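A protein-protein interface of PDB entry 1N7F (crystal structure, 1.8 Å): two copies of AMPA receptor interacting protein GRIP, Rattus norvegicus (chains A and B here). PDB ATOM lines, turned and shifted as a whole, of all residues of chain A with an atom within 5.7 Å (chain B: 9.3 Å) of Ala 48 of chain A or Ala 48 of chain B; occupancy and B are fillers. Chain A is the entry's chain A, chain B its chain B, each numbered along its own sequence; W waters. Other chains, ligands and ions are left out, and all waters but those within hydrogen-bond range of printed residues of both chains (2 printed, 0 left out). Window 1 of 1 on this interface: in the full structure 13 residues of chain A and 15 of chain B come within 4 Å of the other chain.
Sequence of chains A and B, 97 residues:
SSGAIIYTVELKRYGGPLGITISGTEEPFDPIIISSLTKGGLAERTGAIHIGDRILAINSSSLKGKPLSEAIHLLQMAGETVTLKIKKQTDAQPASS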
ATOM      1  N   TYR A   7     -21.723  16.980   8.323  1.00  0.00           N
ATOM      2  CA  TYR A   7     -21.788  17.614   7.016  1.00  0.00           C
ATOM      3  C   TYR A   7     -22.152  19.074   7.195  1.00  0.00           C
ATOM      4  O   TYR A   7     -22.583  19.487   8.269  1.00  0.00           O
ATOM      5  CB  TYR A   7     -22.807  16.908   6.109  1.00  0.00           C
ATOM      6  CG  TYR A   7     -24.256  17.079   6.514  1.00  0.00           C
ATOM      7  CD1 TYR A   7     -25.064  18.030   5.894  1.00  0.00           C
ATOM      8  CD2 TYR A   7     -24.822  16.282   7.509  1.00  0.00           C
ATOM      9  CE1 TYR A   7     -26.401  18.180   6.255  1.00  0.00           C
ATOM     10  CE2 TYR A   7     -26.158  16.428   7.876  1.00  0.00           C
ATOM     11  CZ  TYR A   7     -26.939  17.378   7.244  1.00  0.00           C
ATOM     12  OH  TYR A   7     -28.262  17.527   7.590  1.00  0.00           O
ATOM     13  N   VAL A   9     -24.220  22.526   5.490  1.00  0.00           N
ATOM     14  CA  VAL A   9     -25.223  22.982   4.545  1.00  0.00           C
ATOM     15  C   VAL A   9     -25.262  24.497   4.489  1.00  0.00           C
ATOM     16  O   VAL A   9     -25.079  25.179   5.507  1.00  0.00           O
ATOM     17  CB  VAL A   9     -26.648  22.482   4.912  1.00  0.00           C
ATOM     18  CG1 VAL A   9     -26.718  20.977   4.797  1.00  0.00           C
ATOM     19  CG2 VAL A   9     -27.023  22.924   6.323  1.00  0.00           C
ATOM     20  N   LEU A  11     -27.770  27.428   3.465  1.00  0.00           N
ATOM     21  CA  LEU A  11     -29.158  27.714   3.139  1.00  0.00           C
ATOM     22  C   LEU A  11     -29.404  29.159   2.725  1.00  0.00           C
ATOM     23  O   LEU A  11     -28.974  30.099   3.400  1.00  0.00           O
ATOM     24  CB  LEU A  11     -30.044  27.380   4.342  1.00  0.00           C
ATOM     25  CG  LEU A  11     -30.122  25.905   4.734  1.00  0.00           C
ATOM     26  CD1 LEU A  11     -30.656  25.772   6.156  1.00  0.00           C
ATOM     27  CD2 LEU A  11     -31.007  25.163   3.737  1.00  0.00           C
ATOM     28  N   ALA A  43     -36.410  24.827   5.903  1.00  0.00           N
ATOM     29  CA  ALA A  43     -35.749  23.602   6.336  1.00  0.00           C
ATOM     30  C   ALA A  43     -36.501  22.363   5.855  1.00  0.00           C
ATOM     31  O   ALA A  43     -35.896  21.427   5.334  1.00  0.00           O
ATOM     32  CB  ALA A  43     -35.632  23.581   7.863  1.00  0.00           C
ATOM     33  N   GLU A  44     -37.819  22.360   6.033  1.00  0.00           N
ATOM     34  CA  GLU A  44     -38.633  21.223   5.624  1.00  0.00           C
ATOM     35  C   GLU A  44     -38.634  21.023   4.110  1.00  0.00           C
ATOM     36  O   GLU A  44     -38.457  19.906   3.624  1.00  0.00           O
ATOM     37  CB  GLU A  44     -40.075  21.394   6.115  1.00  0.00           C
ATOM     38  CG  GLU A  44     -40.896  20.117   6.010  1.00  0.00           C
ATOM     39  CD  GLU A  44     -42.283  20.247   6.614  1.00  0.00           C
ATOM     40  OE1 GLU A  44     -43.155  20.880   5.985  1.00  0.00           O
ATOM     41  OE2 GLU A  44     -42.497  19.717   7.725  1.00  0.00           O
ATOM     42  N   THR A  46     -36.434  21.938   1.878  1.00  0.00           N
ATOM     43  CA  THR A  46     -35.146  21.534   1.322  1.00  0.00           C
ATOM     44  C   THR A  46     -34.808  20.111   1.744  1.00  0.00           C
ATOM     45  O   THR A  46     -34.201  19.350   0.982  1.00  0.00           O
ATOM     46  CB  THR A  46     -34.009  22.456   1.799  1.00  0.00           C
ATOM     47  OG1 THR A  46     -33.913  22.395   3.229  1.00  0.00           O
ATOM     48  CG2 THR A  46     -34.264  23.890   1.365  1.00  0.00           C
ATOM     49  N   GLY A  47     -35.220  19.749   2.956  1.00  0.00           N
ATOM     50  CA  GLY A  47     -34.919  18.433   3.484  1.00  0.00           C
ATOM     51  C   GLY A  47     -33.440  18.397   3.834  1.00  0.00           C
ATOM     52  O   GLY A  47     -32.832  17.333   3.915  1.00  0.00           O
ATOM     53  N   ALA A  48     -32.864  19.575   4.054  1.00  0.00           N
ATOM     54  CA  ALA A  48     -31.441  19.704   4.364  1.00  0.00           C
ATOM     55  C   ALA A  48     -31.041  19.384   5.807  1.00  0.00           C
ATOM     56  O   ALA A  48     -29.922  18.925   6.055  1.00  0.00           O
ATOM     57  CB  ALA A  48     -30.966  21.108   4.000  1.00  0.00           C
ATOM     58  N   ILE A  49     -31.944  19.636   6.751  1.00  0.00           N
ATOM     59  CA  ILE A  49     -31.672  19.391   8.168  1.00  0.00           C
ATOM     60  C   ILE A  49     -32.907  18.783   8.825  1.00  0.00           C
ATOM     61  O   ILE A  49     -34.020  18.949   8.324  1.00  0.00           O
ATOM     62  CB  ILE A  49     -31.283  20.709   8.891  1.00  0.00           C
ATOM     63  CG1 ILE A  49     -32.382  21.758   8.695  1.00  0.00           C
ATOM     64  CG2 ILE A  49     -29.952  21.233   8.335  1.00  0.00           C
ATOM     65  CD1 ILE A  49     -32.026  23.149   9.224  1.00  0.00           C
ATOM     66  N   HIS A  50     -32.722  18.083   9.939  1.00  0.00           N
ATOM     67  CA  HIS A  50     -33.856  17.448  10.607  1.00  0.00           C
ATOM     68  C   HIS A  50     -33.799  17.457  12.129  1.00  0.00           C
ATOM     69  O   HIS A  50     -32.753  17.696  12.734  1.00  0.00           O
ATOM     70  CB  HIS A  50     -33.999  16.003  10.124  1.00  0.00           C
ATOM     71  CG  HIS A  50     -34.097  15.872   8.636  1.00  0.00           C
ATOM     72  ND1 HIS A  50     -33.009  16.020   7.803  1.00  0.00           N
ATOM     73  CD2 HIS A  50     -35.162  15.647   7.830  1.00  0.00           C
ATOM     74  CE1 HIS A  50     -33.400  15.893   6.547  1.00  0.00           C
ATOM     75  NE2 HIS A  50     -34.701  15.666   6.535  1.00  0.00           N
ATOM     76  N   ASP A  53     -30.798  16.624  14.858  1.00  0.00           N
ATOM     77  CA  ASP A  53     -29.491  17.045  14.350  1.00  0.00           C
ATOM     78  C   ASP A  53     -28.831  17.999  15.346  1.00  0.00           C
ATOM     79  O   ASP A  53     -29.502  18.860  15.919  1.00  0.00           O
ATOM     80  CB  ASP A  53     -29.638  17.812  13.026  1.00  0.00           C
ATOM     81  CG  ASP A  53     -29.874  16.909  11.819  1.00  0.00           C
ATOM     82  OD1 ASP A  53     -29.776  15.670  11.941  1.00  0.00           O
ATOM     83  OD2 ASP A  53     -30.145  17.463  10.731  1.00  0.00           O
ATOM     84  N   ILE A  86     -23.514  20.408  10.624  1.00  0.00           N
ATOM     85  CA  ILE A  86     -24.409  19.466  11.293  1.00  0.00           C
ATOM     86  C   ILE A  86     -23.811  18.113  11.682  1.00  0.00           C
ATOM     87  O   ILE A  86     -23.088  17.496  10.902  1.00  0.00           O
ATOM     88  CB  ILE A  86     -25.621  19.163  10.375  1.00  0.00           C
ATOM     89  CG1 ILE A  86     -26.315  20.464   9.957  1.00  0.00           C
ATOM     90  CG2 ILE A  86     -26.576  18.208  11.069  1.00  0.00           C
ATOM     91  CD1 ILE A  86     -27.044  21.172  11.074  1.00  0.00           C
ATOM     92  N   ILE B   5     -36.074  26.496  -5.231  1.00  0.00           N
ATOM     93  CA  ILE B   5     -35.343  26.361  -3.975  1.00  0.00           C
ATOM     94  C   ILE B   5     -33.996  25.682  -4.192  1.00  0.00           C
ATOM     95  O   ILE B   5     -33.927  24.532  -4.637  1.00  0.00           O
ATOM     96  CB  ILE B   5     -36.156  25.558  -2.938  1.00  0.00           C
ATOM     97  CG1 ILE B   5     -37.435  26.322  -2.586  1.00  0.00           C
ATOM     98  CG2 ILE B   5     -35.319  25.316  -1.687  1.00  0.00           C
ATOM     99  CD1 ILE B   5     -38.302  25.637  -1.545  1.00  0.00           C
ATOM    100  N   ILE B   6     -32.932  26.407  -3.868  1.00  0.00           N
ATOM    101  CA  ILE B   6     -31.570  25.915  -4.031  1.00  0.00           C
ATOM    102  C   ILE B   6     -30.828  25.947  -2.703  1.00  0.00           C
ATOM    103  O   ILE B   6     -30.991  26.879  -1.921  1.00  0.00           O
ATOM    104  CB  ILE B   6     -30.793  26.797  -5.033  1.00  0.00           C
ATOM    105  CG1 ILE B   6     -31.474  26.750  -6.400  1.00  0.00           C
ATOM    106  CG2 ILE B   6     -29.335  26.343  -5.124  1.00  0.00           C
ATOM    107  CD1 ILE B   6     -30.953  27.790  -7.371  1.00  0.00           C
ATOM    108  N   TYR B   7     -30.022  24.923  -2.448  1.00  0.00           N
ATOM    109  CA  TYR B   7     -29.219  24.872  -1.232  1.00  0.00           C
ATOM    110  C   TYR B   7     -27.947  24.104  -1.558  1.00  0.00           C
ATOM    111  O   TYR B   7     -27.868  23.430  -2.590  1.00  0.00           O
ATOM    112  CB  TYR B   7     -29.993  24.214  -0.077  1.00  0.00           C
ATOM    113  CG  TYR B   7     -30.206  22.719  -0.188  1.00  0.00           C
ATOM    114  CD1 TYR B   7     -29.557  21.843   0.682  1.00  0.00           C
ATOM    115  CD2 TYR B   7     -31.079  22.182  -1.130  1.00  0.00           C
ATOM    116  CE1 TYR B   7     -29.775  20.468   0.623  1.00  0.00           C
ATOM    117  CE2 TYR B   7     -31.304  20.809  -1.200  1.00  0.00           C
ATOM    118  CZ  TYR B   7     -30.648  19.959  -0.319  1.00  0.00           C
ATOM    119  OH  TYR B   7     -30.863  18.604  -0.376  1.00  0.00           O
ATOM    120  N   THR B   8     -26.947  24.208  -0.695  1.00  0.00           N
ATOM    121  CA  THR B   8     -25.679  23.535  -0.943  1.00  0.00           C
ATOM    122  C   THR B   8     -25.296  22.604   0.192  1.00  0.00           C
ATOM    123  O   THR B   8     -25.480  22.939   1.363  1.00  0.00           O
ATOM    124  CB  THR B   8     -24.558  24.571  -1.139  1.00  0.00           C
ATOM    125  OG1 THR B   8     -24.902  25.436  -2.228  1.00  0.00           O
ATOM    126  CG2 THR B   8     -23.241  23.881  -1.440  1.00  0.00           C
ATOM    127  N   VAL B   9     -24.769  21.434  -0.159  1.00  0.00           N
ATOM    128  CA  VAL B   9     -24.353  20.453   0.837  1.00  0.00           C
ATOM    129  C   VAL B   9     -22.892  20.073   0.625  1.00  0.00           C
ATOM    130  O   VAL B   9     -22.474  19.753  -0.492  1.00  0.00           O
ATOM    131  CB  VAL B   9     -25.207  19.162   0.764  1.00  0.00           C
ATOM    132  CG1 VAL B   9     -24.746  18.167   1.826  1.00  0.00           C
ATOM    133  CG2 VAL B   9     -26.679  19.496   0.971  1.00  0.00           C
ATOM    134  N   GLU B  10     -22.121  20.128   1.704  1.00  0.00           N
ATOM    135  CA  GLU B  10     -20.710  19.778   1.660  1.00  0.00           C
ATOM    136  C   GLU B  10     -20.504  18.450   2.383  1.00  0.00           C
ATOM    137  O   GLU B  10     -20.778  18.332   3.583  1.00  0.00           O
ATOM    138  CB  GLU B  10     -19.877  20.877   2.325  1.00  0.00           C
ATOM    139  CG  GLU B  10     -18.408  20.535   2.461  1.00  0.00           C
ATOM    140  CD  GLU B  10     -17.648  21.541   3.305  1.00  0.00           C
ATOM    141  OE1 GLU B  10     -17.505  22.702   2.869  1.00  0.00           O
ATOM    142  OE2 GLU B  10     -17.200  21.172   4.413  1.00  0.00           O
ATOM    143  N   LEU B  11     -20.014  17.454   1.652  1.00  0.00           N
ATOM    144  CA  LEU B  11     -19.786  16.131   2.216  1.00  0.00           C
ATOM    145  C   LEU B  11     -18.304  15.781   2.285  1.00  0.00           C
ATOM    146  O   LEU B  11     -17.533  16.112   1.381  1.00  0.00           O
ATOM    147  CB  LEU B  11     -20.508  15.074   1.374  1.00  0.00           C
ATOM    148  CG  LEU B  11     -22.022  15.212   1.213  1.00  0.00           C
ATOM    149  CD1 LEU B  11     -22.528  14.171   0.222  1.00  0.00           C
ATOM    150  CD2 LEU B  11     -22.694  15.043   2.567  1.00  0.00           C
ATOM    151  N   ILE B  20     -23.836   8.033  -3.838  1.00  0.00           N
ATOM    152  CA  ILE B  20     -24.794   8.691  -4.712  1.00  0.00           C
ATOM    153  C   ILE B  20     -24.636   8.225  -6.151  1.00  0.00           C
ATOM    154  O   ILE B  20     -23.529   7.967  -6.615  1.00  0.00           O
ATOM    155  CB  ILE B  20     -24.595  10.228  -4.698  1.00  0.00           C
ATOM    156  CG1 ILE B  20     -24.806  10.774  -3.286  1.00  0.00           C
ATOM    157  CG2 ILE B  20     -25.550  10.893  -5.673  1.00  0.00           C
ATOM    158  CD1 ILE B  20     -24.582  12.269  -3.169  1.00  0.00           C
ATOM    159  N   ILE B  34     -30.012  13.361  -9.171  1.00  0.00           N
ATOM    160  CA  ILE B  34     -29.625  12.333  -8.222  1.00  0.00           C
ATOM    161  C   ILE B  34     -30.684  11.256  -8.447  1.00  0.00           C
ATOM    162  O   ILE B  34     -31.865  11.479  -8.172  1.00  0.00           O
ATOM    163  CB  ILE B  34     -29.702  12.872  -6.783  1.00  0.00           C
ATOM    164  CG1 ILE B  34     -28.695  14.016  -6.617  1.00  0.00           C
ATOM    165  CG2 ILE B  34     -29.440  11.750  -5.793  1.00  0.00           C
ATOM    166  CD1 ILE B  34     -28.885  14.835  -5.359  1.00  0.00           C
ATOM    167  N   LEU B  37     -29.620   6.356  -4.118  1.00  0.00           N
ATOM    168  CA  LEU B  37     -28.698   6.485  -3.000  1.00  0.00           C
ATOM    169  C   LEU B  37     -28.338   5.100  -2.484  1.00  0.00           C
ATOM    170  O   LEU B  37     -29.198   4.225  -2.378  1.00  0.00           O
ATOM    171  CB  LEU B  37     -29.336   7.293  -1.865  1.00  0.00           C
ATOM    172  CG  LEU B  37     -29.782   8.723  -2.173  1.00  0.00           C
ATOM    173  CD1 LEU B  37     -30.426   9.328  -0.930  1.00  0.00           C
ATOM    174  CD2 LEU B  37     -28.587   9.553  -2.615  1.00  0.00           C
ATOM    175  N   GLY B  41     -25.125   4.306   2.816  1.00  0.00           N
ATOM    176  CA  GLY B  41     -24.036   5.153   2.356  1.00  0.00           C
ATOM    177  C   GLY B  41     -24.024   6.515   3.030  1.00  0.00           C
ATOM    178  O   GLY B  41     -24.975   6.885   3.719  1.00  0.00           O
ATOM    179  N   LEU B  42     -22.949   7.269   2.828  1.00  0.00           N
ATOM    180  CA  LEU B  42     -22.820   8.591   3.436  1.00  0.00           C
ATOM    181  C   LEU B  42     -23.984   9.524   3.107  1.00  0.00           C
ATOM    182  O   LEU B  42     -24.598  10.103   4.004  1.00  0.00           O
ATOM    183  CB  LEU B  42     -21.506   9.247   3.001  1.00  0.00           C
ATOM    184  CG  LEU B  42     -21.300  10.693   3.469  1.00  0.00           C
ATOM    185  CD1 LEU B  42     -21.319  10.758   4.996  1.00  0.00           C
ATOM    186  CD2 LEU B  42     -19.979  11.214   2.938  1.00  0.00           C
ATOM    187  N   ALA B  43     -24.284   9.672   1.821  1.00  0.00           N
ATOM    188  CA  ALA B  43     -25.368  10.551   1.398  1.00  0.00           C
ATOM    189  C   ALA B  43     -26.680  10.211   2.100  1.00  0.00           C
ATOM    190  O   ALA B  43     -27.381  11.099   2.588  1.00  0.00           O
ATOM    191  CB  ALA B  43     -25.549  10.472  -0.111  1.00  0.00           C
ATOM    192  N   GLU B  44     -27.006   8.924   2.158  1.00  0.00           N
ATOM    193  CA  GLU B  44     -28.244   8.497   2.801  1.00  0.00           C
ATOM    194  C   GLU B  44     -28.238   8.780   4.301  1.00  0.00           C
ATOM    195  O   GLU B  44     -29.231   9.249   4.851  1.00  0.00           O
ATOM    196  CB  GLU B  44     -28.490   7.003   2.564  1.00  0.00           C
ATOM    197  CG  GLU B  44     -29.748   6.478   3.249  1.00  0.00           C
ATOM    198  CD  GLU B  44     -30.035   5.019   2.925  1.00  0.00           C
ATOM    199  OE1 GLU B  44     -30.566   4.736   1.827  1.00  0.00           O
ATOM    200  OE2 GLU B  44     -29.721   4.155   3.769  1.00  0.00           O
ATOM    201  N   ARG B  45     -27.115   8.502   4.955  1.00  0.00           N
ATOM    202  CA  ARG B  45     -26.996   8.717   6.393  1.00  0.00           C
ATOM    203  C   ARG B  45     -27.189  10.172   6.810  1.00  0.00           C
ATOM    204  O   ARG B  45     -27.722  10.442   7.886  1.00  0.00           O
ATOM    205  CB  ARG B  45     -25.641   8.216   6.899  1.00  0.00           C
ATOM    206  CG  ARG B  45     -25.437   6.717   6.757  1.00  0.00           C
ATOM    207  CD  ARG B  45     -24.211   6.237   7.526  1.00  0.00           C
ATOM    208  NE  ARG B  45     -24.514   5.854   8.906  1.00  0.00           N
ATOM    209  CZ  ARG B  45     -24.933   6.685   9.859  1.00  0.00           C
ATOM    210  NH1 ARG B  45     -25.107   7.972   9.602  1.00  0.00           N
ATOM    211  NH2 ARG B  45     -25.178   6.224  11.078  1.00  0.00           N
ATOM    212  N   THR B  46     -26.760  11.115   5.975  1.00  0.00           N
ATOM    213  CA  THR B  46     -26.923  12.529   6.316  1.00  0.00           C
ATOM    214  C   THR B  46     -28.391  12.933   6.274  1.00  0.00           C
ATOM    215  O   THR B  46     -28.825  13.813   7.018  1.00  0.00           O
ATOM    216  CB  THR B  46     -26.168  13.462   5.341  1.00  0.00           C
ATOM    217  OG1 THR B  46     -26.747  13.358   4.033  1.00  0.00           O
ATOM    218  CG2 THR B  46     -24.696  13.096   5.283  1.00  0.00           C
ATOM    219  N   GLY B  47     -29.145  12.288   5.388  1.00  0.00           N
ATOM    220  CA  GLY B  47     -30.555  12.600   5.238  1.00  0.00           C
ATOM    221  C   GLY B  47     -30.758  13.920   4.518  1.00  0.00           C
ATOM    222  O   GLY B  47     -31.886  14.381   4.359  1.00  0.00           O
ATOM    223  N   ALA B  48     -29.661  14.523   4.069  1.00  0.00           N
ATOM    224  CA  ALA B  48     -29.713  15.813   3.386  1.00  0.00           C
ATOM    225  C   ALA B  48     -29.631  15.741   1.858  1.00  0.00           C
ATOM    226  O   ALA B  48     -29.598  16.775   1.194  1.00  0.00           O
ATOM    227  CB  ALA B  48     -28.605  16.715   3.919  1.00  0.00           C
ATOM    228  N   ILE B  49     -29.593  14.534   1.308  1.00  0.00           N
ATOM    229  CA  ILE B  49     -29.523  14.352  -0.140  1.00  0.00           C
ATOM    230  C   ILE B  49     -30.751  13.559  -0.581  1.00  0.00           C
ATOM    231  O   ILE B  49     -31.045  12.505  -0.020  1.00  0.00           O
ATOM    232  CB  ILE B  49     -28.247  13.582  -0.542  1.00  0.00           C
ATOM    233  CG1 ILE B  49     -27.009  14.313  -0.012  1.00  0.00           C
ATOM    234  CG2 ILE B  49     -28.175  13.442  -2.055  1.00  0.00           C
ATOM    235  CD1 ILE B  49     -26.871  15.745  -0.505  1.00  0.00           C
ATOM    236  N   HIS B  50     -31.460  14.051  -1.591  1.00  0.00           N
ATOM    237  CA  HIS B  50     -32.671  13.366  -2.027  1.00  0.00           C
ATOM    238  C   HIS B  50     -32.786  13.040  -3.512  1.00  0.00           C
ATOM    239  O   HIS B  50     -32.442  13.849  -4.379  1.00  0.00           O
ATOM    240  CB  HIS B  50     -33.891  14.178  -1.596  1.00  0.00           C
ATOM    241  CG  HIS B  50     -33.888  14.539  -0.143  1.00  0.00           C
ATOM    242  ND1 HIS B  50     -33.167  15.600   0.359  1.00  0.00           N
ATOM    243  CD2 HIS B  50     -34.479  13.948   0.922  1.00  0.00           C
ATOM    244  CE1 HIS B  50     -33.314  15.648   1.671  1.00  0.00           C
ATOM    245  NE2 HIS B  50     -34.104  14.656   2.037  1.00  0.00           N
ATOM    246  N   ILE B  51     -33.298  11.847  -3.788  1.00  0.00           N
ATOM    247  CA  ILE B  51     -33.491  11.389  -5.156  1.00  0.00           C
ATOM    248  C   ILE B  51     -34.456  12.318  -5.881  1.00  0.00           C
ATOM    249  O   ILE B  51     -35.463  12.747  -5.316  1.00  0.00           O
ATOM    250  CB  ILE B  51     -34.063   9.955  -5.183  1.00  0.00           C
ATOM    251  CG1 ILE B  51     -33.040   8.979  -4.597  1.00  0.00           C
ATOM    252  CG2 ILE B  51     -34.437   9.567  -6.607  1.00  0.00           C
ATOM    253  CD1 ILE B  51     -33.515   7.537  -4.549  1.00  0.00           C
ATOM    254  N   ASP B  53     -33.736  15.360  -6.996  1.00  0.00           N
ATOM    255  CA  ASP B  53     -33.194  16.708  -7.009  1.00  0.00           C
ATOM    256  C   ASP B  53     -32.115  16.847  -8.076  1.00  0.00           C
ATOM    257  O   ASP B  53     -31.460  15.876  -8.449  1.00  0.00           O
ATOM    258  CB  ASP B  53     -32.624  17.081  -5.644  1.00  0.00           C
ATOM    259  CG  ASP B  53     -33.706  17.315  -4.608  1.00  0.00           C
ATOM    260  OD1 ASP B  53     -34.868  17.568  -5.002  1.00  0.00           O
ATOM    261  OD2 ASP B  53     -33.390  17.260  -3.405  1.00  0.00           O
ATOM    262  N   LEU B  84     -21.957  20.121  -3.225  1.00  0.00           N
ATOM    263  CA  LEU B  84     -22.997  20.032  -4.240  1.00  0.00           C
ATOM    264  C   LEU B  84     -24.046  21.125  -4.094  1.00  0.00           C
ATOM    265  O   LEU B  84     -24.643  21.282  -3.025  1.00  0.00           O
ATOM    266  CB  LEU B  84     -23.701  18.677  -4.151  1.00  0.00           C
ATOM    267  CG  LEU B  84     -22.836  17.418  -4.176  1.00  0.00           C
ATOM    268  CD1 LEU B  84     -23.706  16.208  -3.895  1.00  0.00           C
ATOM    269  CD2 LEU B  84     -22.137  17.287  -5.525  1.00  0.00           C
ATOM    270  N   ILE B  86     -27.551  22.131  -4.978  1.00  0.00           N
ATOM    271  CA  ILE B  86     -28.740  21.393  -5.375  1.00  0.00           C
ATOM    272  C   ILE B  86     -30.028  22.201  -5.524  1.00  0.00           C
ATOM    273  O   ILE B  86     -30.331  23.070  -4.701  1.00  0.00           O
ATOM    274  CB  ILE B  86     -28.996  20.264  -4.345  1.00  0.00           C
ATOM    275  CG1 ILE B  86     -27.757  19.365  -4.245  1.00  0.00           C
ATOM    276  CG2 ILE B  86     -30.237  19.472  -4.721  1.00  0.00           C
ATOM    277  CD1 ILE B  86     -27.788  18.393  -3.086  1.00  0.00           C
ATOM    278  N   LYS B  88     -34.119  21.842  -5.698  1.00  0.00           N
ATOM    279  CA  LYS B  88     -35.200  20.918  -5.388  1.00  0.00           C
ATOM    280  C   LYS B  88     -36.052  20.646  -6.629  1.00  0.00           C
ATOM    281  O   LYS B  88     -36.279  21.542  -7.442  1.00  0.00           O
ATOM    282  CB  LYS B  88     -36.077  21.491  -4.270  1.00  0.00           C
ATOM    283  CG  LYS B  88     -35.325  21.770  -2.975  1.00  0.00           C
ATOM    284  CD  LYS B  88     -34.679  20.508  -2.422  1.00  0.00           C
ATOM    285  CE  LYS B  88     -35.710  19.470  -2.010  1.00  0.00           C
ATOM    286  NZ  LYS B  88     -35.059  18.242  -1.476  1.00  0.00           N
HETATM  287  O   HOH W   1     -36.436  15.465   4.348  1.00  0.00           O
HETATM  288  O   HOH W   2     -30.349  16.016   8.526  1.00  0.00           O
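The side-chain amino group (NZ) of Lys 88 of chain B lies within hydrogen-bond range of the backbone carbonyl oxygen (O) of Thr 46 of chain A (2.8 Å).
The backbone carbonyl oxygen of Gly 47 of chain B lies close to the backbone carbonyl oxygen of Gly 47 of chain A, at 3.1 Å.
The backbone carbonyl oxygen of Ala 43 of chain B sits at hydrogen-bond distance from the side-chain hydroxyl of Thr 46 of chain B (2.8 Å).
N of His 50 of chain A is in hydrogen-bond range of OD2 of Asp 53 of chain A, 2.8 Å away.
The side-chain hydroxyl (OG1) of Thr 46 of chain A lies close to the backbone NH (N) of Ala 48 of chain A.
The side-chain hydroxyl of Tyr 7 of chain A is in hydrogen-bond range of the backbone carbonyl oxygen of Ala 48 of chain A (2.7 Å).
The side-chain amino group (NZ) of Lys 88 of chain B is in salt-bridge range of the side-chain carboxylate (OD2) of Asp 53 of chain B, at 2.7 Å.
The side-chain hydroxyl of Thr 46 of chain A lies within hydrogen-bond range of the backbone carbonyl oxygen of Ala 43 of chain A.
Of chain B, only Tyr 7 (3.6 Å) and Ala 48 (3.3 Å) come within 4 Å of Ala 48 of chain A.
Ala 48 of chain B touches just these residues of chain A: Tyr 7, Gly 47 and Ala 48.
Printed residues of chain B within 4 Å of Thr 46 of chain A: Ile 5, Tyr 7, His 50 and Lys 88.
Of chain B, only Gly 47 (3.1 Å), Ala 48 (3.5 Å) and His 50 (2.8 Å) come within 4 Å of Gly 47 of chain A.
Ile 49 of chain A touches none of the printed residues of chain B.
Printed residues of chain A within 4 Å of Thr 46 of chain B: Tyr 7 (3.8 Å).
Printed residues of chain A within 4 Å of His 50 of chain B: Thr 46 (3.9 Å) and Gly 47 (2.8 Å).
Of the printed residues of chain A, Thr 8 of chain B touches Val 9.
Of the printed residues of chain B, His 50 of chain A touches Gly 47 (3.1 Å).
The nearest residue of chain B that does not touch Ala 48 of chain A is His 50 of chain B (4.6 Å).
Hydrophobic or aromatic side chains of chain A within 4 Å of the printed part of chain B: Tyr 7, Val 9, Ala 48 and His 50.
Among the printed residues, 14 pairs touch across the chains.
Water W2 lies within hydrogen-bond range of OD2 of Asp 53 of chain A, OH of Tyr 7 of chain A, ND1 of His 50 of chain A and O of Thr 46 of chain B.
Water W1 bridges NE2 of His 50 of chain A (2.8 Å) and NE2 of His 50 of chain B (3.4 Å).
Among the printed residues, merely in contact across the chains: Gly 47 of chain A with His 50 of chain B (2.8 Å), His 50 of chain A with Gly 47 of chain B (3.1 Å), Val 9 of chain A with Thr 8 of chain B (3.2 Å), Ala 48 of chain A with Ala 48 of chain B (3.3 Å), Gly 47 of chain A with Ala 48 of chain B (3.5 Å), Tyr 7 of chain A with Ala 48 of chain B (3.5 Å), Thr 46 of chain A with Ile 5 of chain B (3.5 Å), Tyr 7 of chain A with Glu 10 of chain B (3.5 Å), Ala 48 of chain A with Tyr 7 of chain B (3.6 Å), Thr 46 of chain A with Tyr 7 of chain B (3.7 Å), Tyr 7 of chain A with Thr 46 of chain B (3.8 Å) and Thr 46 of chain A with His 50 of chain B (3.9 Å).
Tyr 7 of chain A touches Thr 46 of chain B, and with the chains exchanged Thr 46 of chain A touches Tyr 7 of chain B.
Thr 46 of chain A touches His 50 of chain B, but with the chains exchanged His 50 of chain A does not touch Thr 46 of chain B (4.8 Å).
Gly 47 of chain A touches His 50 of chain B, and with the chains exchanged His 50 of chain A touches Gly 47 of chain B.
Ala 48 of chain B touches its own counterpart, Ala 48 of chain A.
Of the 14 pairs that touch across the chains among the printed residues, 8 have their exchanged pair printed and touching as well.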
